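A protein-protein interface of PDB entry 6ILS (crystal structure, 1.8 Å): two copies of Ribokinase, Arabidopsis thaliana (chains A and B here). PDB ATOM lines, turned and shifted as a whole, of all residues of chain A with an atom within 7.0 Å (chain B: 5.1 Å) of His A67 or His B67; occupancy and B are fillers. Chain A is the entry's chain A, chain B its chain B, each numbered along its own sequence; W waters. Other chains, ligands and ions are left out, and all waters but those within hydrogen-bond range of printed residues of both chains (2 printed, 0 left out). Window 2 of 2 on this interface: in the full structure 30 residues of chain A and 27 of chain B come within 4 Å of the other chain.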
ATOM      1  N   ASN A  12      17.124  26.473   3.504  1.00  0.00           N
ATOM      2  CA  ASN A  12      18.091  27.558   3.333  1.00  0.00           C
ATOM      3  C   ASN A  12      18.502  28.177   4.651  1.00  0.00           C
ATOM      4  O   ASN A  12      17.678  28.308   5.537  1.00  0.00           O
ATOM      5  CB  ASN A  12      17.516  28.675   2.466  1.00  0.00           C
ATOM      6  CG  ASN A  12      17.440  28.309   1.025  1.00  0.00           C
ATOM      7  OD1 ASN A  12      18.334  27.656   0.491  1.00  0.00           O
ATOM      8  ND2 ASN A  12      16.377  28.755   0.360  1.00  0.00           N
ATOM      9  N   ALA A  13      19.762  28.580   4.765  1.00  0.00           N
ATOM     10  CA  ALA A  13      20.147  29.497   5.825  1.00  0.00           C
ATOM     11  C   ALA A  13      19.946  30.907   5.292  1.00  0.00           C
ATOM     12  O   ALA A  13      20.512  31.265   4.272  1.00  0.00           O
ATOM     13  CB  ALA A  13      21.591  29.278   6.252  1.00  0.00           C
ATOM     14  N   ASP A  14      19.124  31.693   5.975  1.00  0.00           N
ATOM     15  CA  ASP A  14      18.890  33.074   5.588  1.00  0.00           C
ATOM     16  C   ASP A  14      19.810  33.976   6.394  1.00  0.00           C
ATOM     17  O   ASP A  14      19.671  34.082   7.609  1.00  0.00           O
ATOM     18  CB  ASP A  14      17.428  33.459   5.799  1.00  0.00           C
ATOM     19  CG  ASP A  14      16.483  32.730   4.839  1.00  0.00           C
ATOM     20  OD1 ASP A  14      16.876  32.496   3.674  1.00  0.00           O
ATOM     21  OD2 ASP A  14      15.360  32.391   5.256  1.00  0.00           O
ATOM     22  N   ILE A  15      20.748  34.601   5.695  1.00  0.00           N
ATOM     23  CA  ILE A  15      21.778  35.421   6.311  1.00  0.00           C
ATOM     24  C   ILE A  15      21.443  36.898   6.142  1.00  0.00           C
ATOM     25  O   ILE A  15      21.745  37.502   5.117  1.00  0.00           O
ATOM     26  CB  ILE A  15      23.133  35.115   5.709  1.00  0.00           C
ATOM     27  CG1 ILE A  15      23.413  33.615   5.812  1.00  0.00           C
ATOM     28  CG2 ILE A  15      24.229  35.920   6.420  1.00  0.00           C
ATOM     29  CD1 ILE A  15      24.490  33.144   4.908  1.00  0.00           C
ATOM     30  N   GLN A  35      22.149  38.384  11.472  1.00  0.00           N
ATOM     31  CA  GLN A  35      21.744  37.113  12.047  1.00  0.00           C
ATOM     32  C   GLN A  35      21.495  36.103  10.939  1.00  0.00           C
ATOM     33  O   GLN A  35      21.118  36.467   9.820  1.00  0.00           O
ATOM     34  CB  GLN A  35      20.508  37.271  12.935  1.00  0.00           C
ATOM     35  CG  GLN A  35      19.403  38.112  12.335  1.00  0.00           C
ATOM     36  CD  GLN A  35      18.229  38.300  13.287  1.00  0.00           C
ATOM     37  OE1 GLN A  35      17.912  37.415  14.087  1.00  0.00           O
ATOM     38  NE2 GLN A  35      17.581  39.459  13.207  1.00  0.00           N
ATOM     39  N   THR A  36      21.736  34.838  11.259  1.00  0.00           N
ATOM     40  CA  THR A  36      21.544  33.757  10.301  1.00  0.00           C
ATOM     41  C   THR A  36      20.463  32.818  10.824  1.00  0.00           C
ATOM     42  O   THR A  36      20.535  32.328  11.949  1.00  0.00           O
ATOM     43  CB  THR A  36      22.848  33.007  10.042  1.00  0.00           C
ATOM     44  OG1 THR A  36      23.839  33.930   9.572  1.00  0.00           O
ATOM     45  CG2 THR A  36      22.639  31.933   8.990  1.00  0.00           C
ATOM     46  N   ALA A  38      17.273  29.751  10.022  1.00  0.00           N
ATOM     47  CA  ALA A  38      16.796  28.628   9.230  1.00  0.00           C
ATOM     48  C   ALA A  38      15.586  29.045   8.424  1.00  0.00           C
ATOM     49  O   ALA A  38      14.678  29.694   8.943  1.00  0.00           O
ATOM     50  CB  ALA A  38      16.460  27.443  10.131  1.00  0.00           C
ATOM     51  N   LEU A  62      21.058  18.824   2.200  1.00  0.00           N
ATOM     52  CA  LEU A  62      21.882  19.800   2.888  1.00  0.00           C
ATOM     53  C   LEU A  62      23.335  19.591   2.535  1.00  0.00           C
ATOM     54  O   LEU A  62      23.703  18.530   2.039  1.00  0.00           O
ATOM     55  CB  LEU A  62      21.720  19.667   4.407  1.00  0.00           C
ATOM     56  CG  LEU A  62      20.314  19.751   4.975  1.00  0.00           C
ATOM     57  CD1 LEU A  62      20.351  19.456   6.450  1.00  0.00           C
ATOM     58  CD2 LEU A  62      19.694  21.133   4.690  1.00  0.00           C
ATOM     59  N   GLY A  63      24.171  20.576   2.852  1.00  0.00           N
ATOM     60  CA  GLY A  63      25.605  20.350   2.848  1.00  0.00           C
ATOM     61  C   GLY A  63      26.054  19.862   4.222  1.00  0.00           C
ATOM     62  O   GLY A  63      25.365  20.069   5.226  1.00  0.00           O
ATOM     63  N   GLU A  64      27.202  19.194   4.272  1.00  0.00           N
ATOM     64  CA  GLU A  64      27.832  18.857   5.540  1.00  0.00           C
ATOM     65  C   GLU A  64      28.605  20.073   6.037  1.00  0.00           C
ATOM     66  O   GLU A  64      29.838  20.101   5.982  1.00  0.00           O
ATOM     67  CB  GLU A  64      28.759  17.650   5.388  1.00  0.00           C
ATOM     68  CG  GLU A  64      28.024  16.351   5.089  1.00  0.00           C
ATOM     69  CD  GLU A  64      28.943  15.262   4.553  1.00  0.00           C
ATOM     70  OE1 GLU A  64      28.422  14.258   4.019  1.00  0.00           O
ATOM     71  OE2 GLU A  64      30.181  15.411   4.664  1.00  0.00           O
ATOM     72  N   ASP A  65      27.867  21.079   6.495  1.00  0.00           N
ATOM     73  CA  ASP A  65      28.432  22.352   6.929  1.00  0.00           C
ATOM     74  C   ASP A  65      27.599  22.937   8.057  1.00  0.00           C
ATOM     75  O   ASP A  65      26.614  22.340   8.472  1.00  0.00           O
ATOM     76  CB  ASP A  65      28.513  23.344   5.758  1.00  0.00           C
ATOM     77  CG  ASP A  65      27.170  23.558   5.071  1.00  0.00           C
ATOM     78  OD1 ASP A  65      26.137  23.133   5.633  1.00  0.00           O
ATOM     79  OD2 ASP A  65      27.152  24.155   3.966  1.00  0.00           O
ATOM     80  N   ALA A  66      27.970  24.124   8.527  1.00  0.00           N
ATOM     81  CA  ALA A  66      27.313  24.725   9.688  1.00  0.00           C
ATOM     82  C   ALA A  66      25.855  25.093   9.412  1.00  0.00           C
ATOM     83  O   ALA A  66      25.011  24.993  10.292  1.00  0.00           O
ATOM     84  CB  ALA A  66      28.078  25.966  10.142  1.00  0.00           C
ATOM     85  N   HIS A  67      25.573  25.552   8.195  1.00  0.00           N
ATOM     86  CA  HIS A  67      24.203  25.933   7.855  1.00  0.00           C
ATOM     87  C   HIS A  67      23.292  24.710   7.795  1.00  0.00           C
ATOM     88  O   HIS A  67      22.110  24.814   8.077  1.00  0.00           O
ATOM     89  CB  HIS A  67      24.177  26.706   6.548  1.00  0.00           C
ATOM     90  CG  HIS A  67      24.873  28.027   6.641  1.00  0.00           C
ATOM     91  ND1 HIS A  67      25.385  28.684   5.544  1.00  0.00           N
ATOM     92  CD2 HIS A  67      25.160  28.801   7.715  1.00  0.00           C
ATOM     93  CE1 HIS A  67      25.961  29.808   5.939  1.00  0.00           C
ATOM     94  NE2 HIS A  67      25.836  29.904   7.251  1.00  0.00           N
ATOM     95  N   GLY A  68      23.850  23.560   7.437  1.00  0.00           N
ATOM     96  CA  GLY A  68      23.108  22.311   7.497  1.00  0.00           C
ATOM     97  C   GLY A  68      22.762  21.928   8.931  1.00  0.00           C
ATOM     98  O   GLY A  68      21.642  21.524   9.245  1.00  0.00           O
ATOM     99  N   LYS A  69      23.726  22.061   9.834  1.00  0.00           N
ATOM    100  CA  LYS A  69      23.434  21.786  11.237  1.00  0.00           C
ATOM    101  C   LYS A  69      22.392  22.766  11.801  1.00  0.00           C
ATOM    102  O   LYS A  69      21.553  22.400  12.641  1.00  0.00           O
ATOM    103  CB  LYS A  69      24.728  21.844  12.055  1.00  0.00           C
ATOM    104  CG  LYS A  69      25.846  21.026  11.441  1.00  0.00           C
ATOM    105  CD  LYS A  69      26.973  20.760  12.438  1.00  0.00           C
ATOM    106  CE  LYS A  69      26.563  19.741  13.491  1.00  0.00           C
ATOM    107  NZ  LYS A  69      27.722  19.303  14.327  1.00  0.00           N
ATOM    108  N   LEU A  70      22.458  24.009  11.335  1.00  0.00           N
ATOM    109  CA  LEU A  70      21.521  25.056  11.745  1.00  0.00           C
ATOM    110  C   LEU A  70      20.075  24.637  11.432  1.00  0.00           C
ATOM    111  O   LEU A  70      19.172  24.725  12.276  1.00  0.00           O
ATOM    112  CB  LEU A  70      21.886  26.369  11.040  1.00  0.00           C
ATOM    113  CG  LEU A  70      21.101  27.604  11.456  1.00  0.00           C
ATOM    114  CD1 LEU A  70      22.019  28.802  11.593  1.00  0.00           C
ATOM    115  CD2 LEU A  70      20.037  27.882  10.432  1.00  0.00           C
ATOM    116  N   ILE A  71      19.878  24.143  10.217  1.00  0.00           N
ATOM    117  CA  ILE A  71      18.559  23.697   9.769  1.00  0.00           C
ATOM    118  C   ILE A  71      18.108  22.487  10.570  1.00  0.00           C
ATOM    119  O   ILE A  71      16.994  22.437  11.090  1.00  0.00           O
ATOM    120  CB  ILE A  71      18.580  23.317   8.260  1.00  0.00           C
ATOM    121  CG1 ILE A  71      19.053  24.493   7.406  1.00  0.00           C
ATOM    122  CG2 ILE A  71      17.212  22.801   7.820  1.00  0.00           C
ATOM    123  CD1 ILE A  71      18.111  25.629   7.386  1.00  0.00           C
ATOM    124  N   ALA A  72      18.984  21.497  10.669  1.00  0.00           N
ATOM    125  CA  ALA A  72      18.622  20.268  11.353  1.00  0.00           C
ATOM    126  C   ALA A  72      18.251  20.566  12.803  1.00  0.00           C
ATOM    127  O   ALA A  72      17.313  19.993  13.343  1.00  0.00           O
ATOM    128  CB  ALA A  72      19.759  19.256  11.275  1.00  0.00           C
ATOM    129  N   PRO A  94      27.478  23.183  -0.688  1.00  0.00           N
ATOM    130  CA  PRO A  94      27.049  23.922   0.503  1.00  0.00           C
ATOM    131  C   PRO A  94      25.547  23.796   0.711  1.00  0.00           C
ATOM    132  O   PRO A  94      24.793  23.676  -0.273  1.00  0.00           O
ATOM    133  CB  PRO A  94      27.411  25.366   0.169  1.00  0.00           C
ATOM    134  CG  PRO A  94      27.282  25.424  -1.350  1.00  0.00           C
ATOM    135  CD  PRO A  94      27.768  24.077  -1.827  1.00  0.00           C
ATOM    136  N   THR A  95      25.119  23.837   1.966  1.00  0.00           N
ATOM    137  CA  THR A  95      23.711  24.047   2.267  1.00  0.00           C
ATOM    138  C   THR A  95      23.273  25.298   1.515  1.00  0.00           C
ATOM    139  O   THR A  95      24.028  26.280   1.418  1.00  0.00           O
ATOM    140  CB  THR A  95      23.473  24.193   3.784  1.00  0.00           C
ATOM    141  OG1 THR A  95      23.807  22.963   4.432  1.00  0.00           O
ATOM    142  CG2 THR A  95      22.014  24.531   4.097  1.00  0.00           C
ATOM    143  N   GLY A  96      22.066  25.262   0.957  1.00  0.00           N
ATOM    144  CA  GLY A  96      21.541  26.413   0.259  1.00  0.00           C
ATOM    145  C   GLY A  96      21.449  27.612   1.188  1.00  0.00           C
ATOM    146  O   GLY A  96      21.139  27.477   2.375  1.00  0.00           O
ATOM    147  N   HIS A  97      21.730  28.797   0.665  1.00  0.00           N
ATOM    148  CA  HIS A  97      21.606  29.990   1.493  1.00  0.00           C
ATOM    149  C   HIS A  97      21.332  31.269   0.709  1.00  0.00           C
ATOM    150  O   HIS A  97      21.507  31.343  -0.507  1.00  0.00           O
ATOM    151  CB  HIS A  97      22.856  30.185   2.367  1.00  0.00           C
ATOM    152  CG  HIS A  97      24.155  30.103   1.625  1.00  0.00           C
ATOM    153  ND1 HIS A  97      24.599  28.945   1.023  1.00  0.00           N
ATOM    154  CD2 HIS A  97      25.141  31.016   1.451  1.00  0.00           C
ATOM    155  CE1 HIS A  97      25.783  29.158   0.475  1.00  0.00           C
ATOM    156  NE2 HIS A  97      26.134  30.408   0.721  1.00  0.00           N
ATOM    157  N   ALA B  13      32.784  33.330  11.191  1.00  0.00           N
ATOM    158  CA  ALA B  13      32.454  32.411  10.111  1.00  0.00           C
ATOM    159  C   ALA B  13      32.569  33.220   8.824  1.00  0.00           C
ATOM    160  O   ALA B  13      31.958  34.271   8.695  1.00  0.00           O
ATOM    161  CB  ALA B  13      31.054  31.829  10.278  1.00  0.00           C
ATOM    162  N   ILE B  15      31.665  33.673   5.156  1.00  0.00           N
ATOM    163  CA  ILE B  15      30.652  33.255   4.186  1.00  0.00           C
ATOM    164  C   ILE B  15      31.025  33.731   2.777  1.00  0.00           C
ATOM    165  O   ILE B  15      30.761  34.873   2.413  1.00  0.00           O
ATOM    166  CB  ILE B  15      29.257  33.804   4.517  1.00  0.00           C
ATOM    167  CG1 ILE B  15      28.906  33.631   6.003  1.00  0.00           C
ATOM    168  CG2 ILE B  15      28.209  33.119   3.646  1.00  0.00           C
ATOM    169  CD1 ILE B  15      28.587  32.241   6.382  1.00  0.00           C
ATOM    170  N   THR B  36      31.192  28.045   3.574  1.00  0.00           N
ATOM    171  CA  THR B  36      31.332  28.715   4.870  1.00  0.00           C
ATOM    172  C   THR B  36      32.485  28.087   5.628  1.00  0.00           C
ATOM    173  O   THR B  36      32.492  26.876   5.864  1.00  0.00           O
ATOM    174  CB  THR B  36      30.049  28.625   5.716  1.00  0.00           C
ATOM    175  OG1 THR B  36      29.028  29.432   5.117  1.00  0.00           O
ATOM    176  CG2 THR B  36      30.316  29.137   7.129  1.00  0.00           C
ATOM    177  N   ASP B  65      25.749  29.391  18.774  1.00  0.00           N
ATOM    178  CA  ASP B  65      25.080  29.137  17.500  1.00  0.00           C
ATOM    179  C   ASP B  65      25.922  28.211  16.632  1.00  0.00           C
ATOM    180  O   ASP B  65      26.976  27.745  17.052  1.00  0.00           O
ATOM    181  CB  ASP B  65      24.775  30.453  16.760  1.00  0.00           C
ATOM    182  CG  ASP B  65      25.996  31.387  16.650  1.00  0.00           C
ATOM    183  OD1 ASP B  65      27.137  30.891  16.638  1.00  0.00           O
ATOM    184  OD2 ASP B  65      25.790  32.620  16.572  1.00  0.00           O
ATOM    185  N   ALA B  66      25.447  27.935  15.419  1.00  0.00           N
ATOM    186  CA  ALA B  66      26.119  26.992  14.538  1.00  0.00           C
ATOM    187  C   ALA B  66      27.489  27.511  14.069  1.00  0.00           C
ATOM    188  O   ALA B  66      28.434  26.736  13.928  1.00  0.00           O
ATOM    189  CB  ALA B  66      25.222  26.674  13.324  1.00  0.00           C
ATOM    190  N   HIS B  67      27.576  28.813  13.821  1.00  0.00           N
ATOM    191  CA  HIS B  67      28.852  29.447  13.453  1.00  0.00           C
ATOM    192  C   HIS B  67      29.878  29.331  14.590  1.00  0.00           C
ATOM    193  O   HIS B  67      31.077  29.112  14.349  1.00  0.00           O
ATOM    194  CB  HIS B  67      28.641  30.917  13.108  1.00  0.00           C
ATOM    195  CG  HIS B  67      27.971  31.148  11.788  1.00  0.00           C
ATOM    196  ND1 HIS B  67      27.344  32.335  11.477  1.00  0.00           N
ATOM    197  CD2 HIS B  67      27.851  30.362  10.691  1.00  0.00           C
ATOM    198  CE1 HIS B  67      26.855  32.268  10.252  1.00  0.00           C
ATOM    199  NE2 HIS B  67      27.156  31.086   9.749  1.00  0.00           N
ATOM    200  N   GLY B  68      29.395  29.489  15.818  1.00  0.00           N
ATOM    201  CA  GLY B  68      30.223  29.332  17.001  1.00  0.00           C
ATOM    202  C   GLY B  68      30.780  27.935  17.095  1.00  0.00           C
ATOM    203  O   GLY B  68      31.950  27.739  17.419  1.00  0.00           O
ATOM    204  N   LYS B  69      29.931  26.949  16.812  1.00  0.00           N
ATOM    205  CA  LYS B  69      30.332  25.556  16.841  1.00  0.00           C
ATOM    206  C   LYS B  69      31.359  25.229  15.762  1.00  0.00           C
ATOM    207  O   LYS B  69      32.283  24.446  15.993  1.00  0.00           O
ATOM    208  CB  LYS B  69      29.108  24.646  16.678  1.00  0.00           C
ATOM    209  CG  LYS B  69      29.352  23.220  17.150  1.00  0.00           C
ATOM    210  CD  LYS B  69      28.232  22.777  18.096  1.00  0.00           C
ATOM    211  CE  LYS B  69      28.729  21.818  19.169  1.00  0.00           C
ATOM    212  NZ  LYS B  69      27.657  21.492  20.164  1.00  0.00           N
ATOM    213  N   LEU B  70      31.165  25.809  14.584  1.00  0.00           N
ATOM    214  CA  LEU B  70      32.108  25.675  13.481  1.00  0.00           C
ATOM    215  C   LEU B  70      33.514  26.072  13.937  1.00  0.00           C
ATOM    216  O   LEU B  70      34.484  25.365  13.699  1.00  0.00           O
ATOM    217  CB  LEU B  70      31.656  26.544  12.309  1.00  0.00           C
ATOM    218  CG  LEU B  70      32.591  26.777  11.122  1.00  0.00           C
ATOM    219  CD1 LEU B  70      32.820  25.483  10.352  1.00  0.00           C
ATOM    220  CD2 LEU B  70      32.002  27.872  10.233  1.00  0.00           C
ATOM    221  N   ILE B  71      33.594  27.215  14.595  1.00  0.00           N
ATOM    222  CA  ILE B  71      34.873  27.738  15.072  1.00  0.00           C
ATOM    223  C   ILE B  71      35.519  26.802  16.089  1.00  0.00           C
ATOM    224  O   ILE B  71      36.684  26.438  15.970  1.00  0.00           O
ATOM    225  CB  ILE B  71      34.709  29.113  15.741  1.00  0.00           C
ATOM    226  CG1 ILE B  71      33.995  30.114  14.823  1.00  0.00           C
ATOM    227  CG2 ILE B  71      36.060  29.619  16.232  1.00  0.00           C
ATOM    228  CD1 ILE B  71      34.711  30.393  13.541  1.00  0.00           C
ATOM    229  N   THR B  95      27.746  34.821  16.841  1.00  0.00           N
ATOM    230  CA  THR B  95      29.158  34.693  16.452  1.00  0.00           C
ATOM    231  C   THR B  95      29.404  35.658  15.296  1.00  0.00           C
ATOM    232  O   THR B  95      28.569  35.771  14.396  1.00  0.00           O
ATOM    233  CB  THR B  95      29.495  33.233  16.046  1.00  0.00           C
ATOM    234  OG1 THR B  95      29.292  32.371  17.173  1.00  0.00           O
ATOM    235  CG2 THR B  95      30.942  33.074  15.532  1.00  0.00           C
ATOM    236  N   HIS B  97      30.644  37.254  11.853  1.00  0.00           N
ATOM    237  CA  HIS B  97      30.779  36.643  10.548  1.00  0.00           C
ATOM    238  C   HIS B  97      31.055  37.702   9.497  1.00  0.00           C
ATOM    239  O   HIS B  97      30.862  38.901   9.733  1.00  0.00           O
ATOM    240  CB  HIS B  97      29.529  35.805  10.192  1.00  0.00           C
ATOM    241  CG  HIS B  97      28.224  36.486  10.467  1.00  0.00           C
ATOM    242  ND1 HIS B  97      27.734  36.672  11.741  1.00  0.00           N
ATOM    243  CD2 HIS B  97      27.275  36.969   9.627  1.00  0.00           C
ATOM    244  CE1 HIS B  97      26.558  37.276  11.676  1.00  0.00           C
ATOM    245  NE2 HIS B  97      26.253  37.458  10.403  1.00  0.00           N
HETATM  246  O   HOH W   1      29.590  25.639   3.059  1.00  0.00           O
HETATM  247  O   HOH W   2      30.879  25.004   7.478  1.00  0.00           O
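NE2 of His B67 is in hydrogen-bond range of NE2 of His A67 (3.1 Å).
Ile A15 touches Ile B15 (CD1 to CG2, 3.9 Å).
His B67 touches Thr A36 (CE1 to OG1, 3.5 Å).
O of Ala A66 touches CB of Ala B66, 3.5 Å away.
His A67 touches Ile B15 (CE1 to CD1, 3.6 Å).
CE1 of His A67 touches OG1 of Thr B36, 3.2 Å away.
Printed residues of chain B within 4 Å of Thr A36: His B67 (3.5 Å).
Printed residues of chain B within 4 Å of Ala A66: Ala B66 (3.5 Å).
Of chain B, only Ile B15, Thr B36 and His B67 come within 4 Å of His A67.
His A97 touches none of the printed residues of chain B.
Of the printed residues of chain A, Ala B66 touches Ala A66.
His B67 touches two residues of chain A.
The nearest printed residue of chain B that does not touch His A67 is Ala B66 (5.3 Å).
The nearest printed residue of chain B that does not touch Ala A66 is Leu B70 (4.2 Å).
Hydrophobic or aromatic side chains of chain A within 4 Å of the printed part of chain B: Ile A15, Ala A66 and His A67.
Of the 12 printed residues of chain B, 4 touch a printed residue of chain A.
Hydrophobic or aromatic side chains of chain B within 4 Å of the printed part of chain A: Ile B15, Ala B66 and His B67.
Among the printed residues, no Asp or Glu carboxylate lies within 4 Å of a Lys or Arg side-chain nitrogen of the other chain.
Ile A15 touches its own counterpart, Ile B15.
Thr A36 touches His B67, and with the chains exchanged His A67 touches Thr B36.
Ala A66 touches its own counterpart, Ala B66.
His A67 touches Ile B15, but with the chains exchanged Ile A15 does not touch His B67 (5.8 Å).
Positions printed for both chains: 13, 15, 36, 65, 66, 67, 68, 69, 70, 71, 95 and 97.
Water W1 lies within hydrogen-bond range of the backbone NH of Thr B36 (2.9 Å) and the side-chain carboxylate of Asp A65 (3.0 Å).
Water W2 lies within hydrogen-bond range of the backbone carbonyl oxygen (O) of Thr B36 and the backbone NH (N) of Ala A66.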
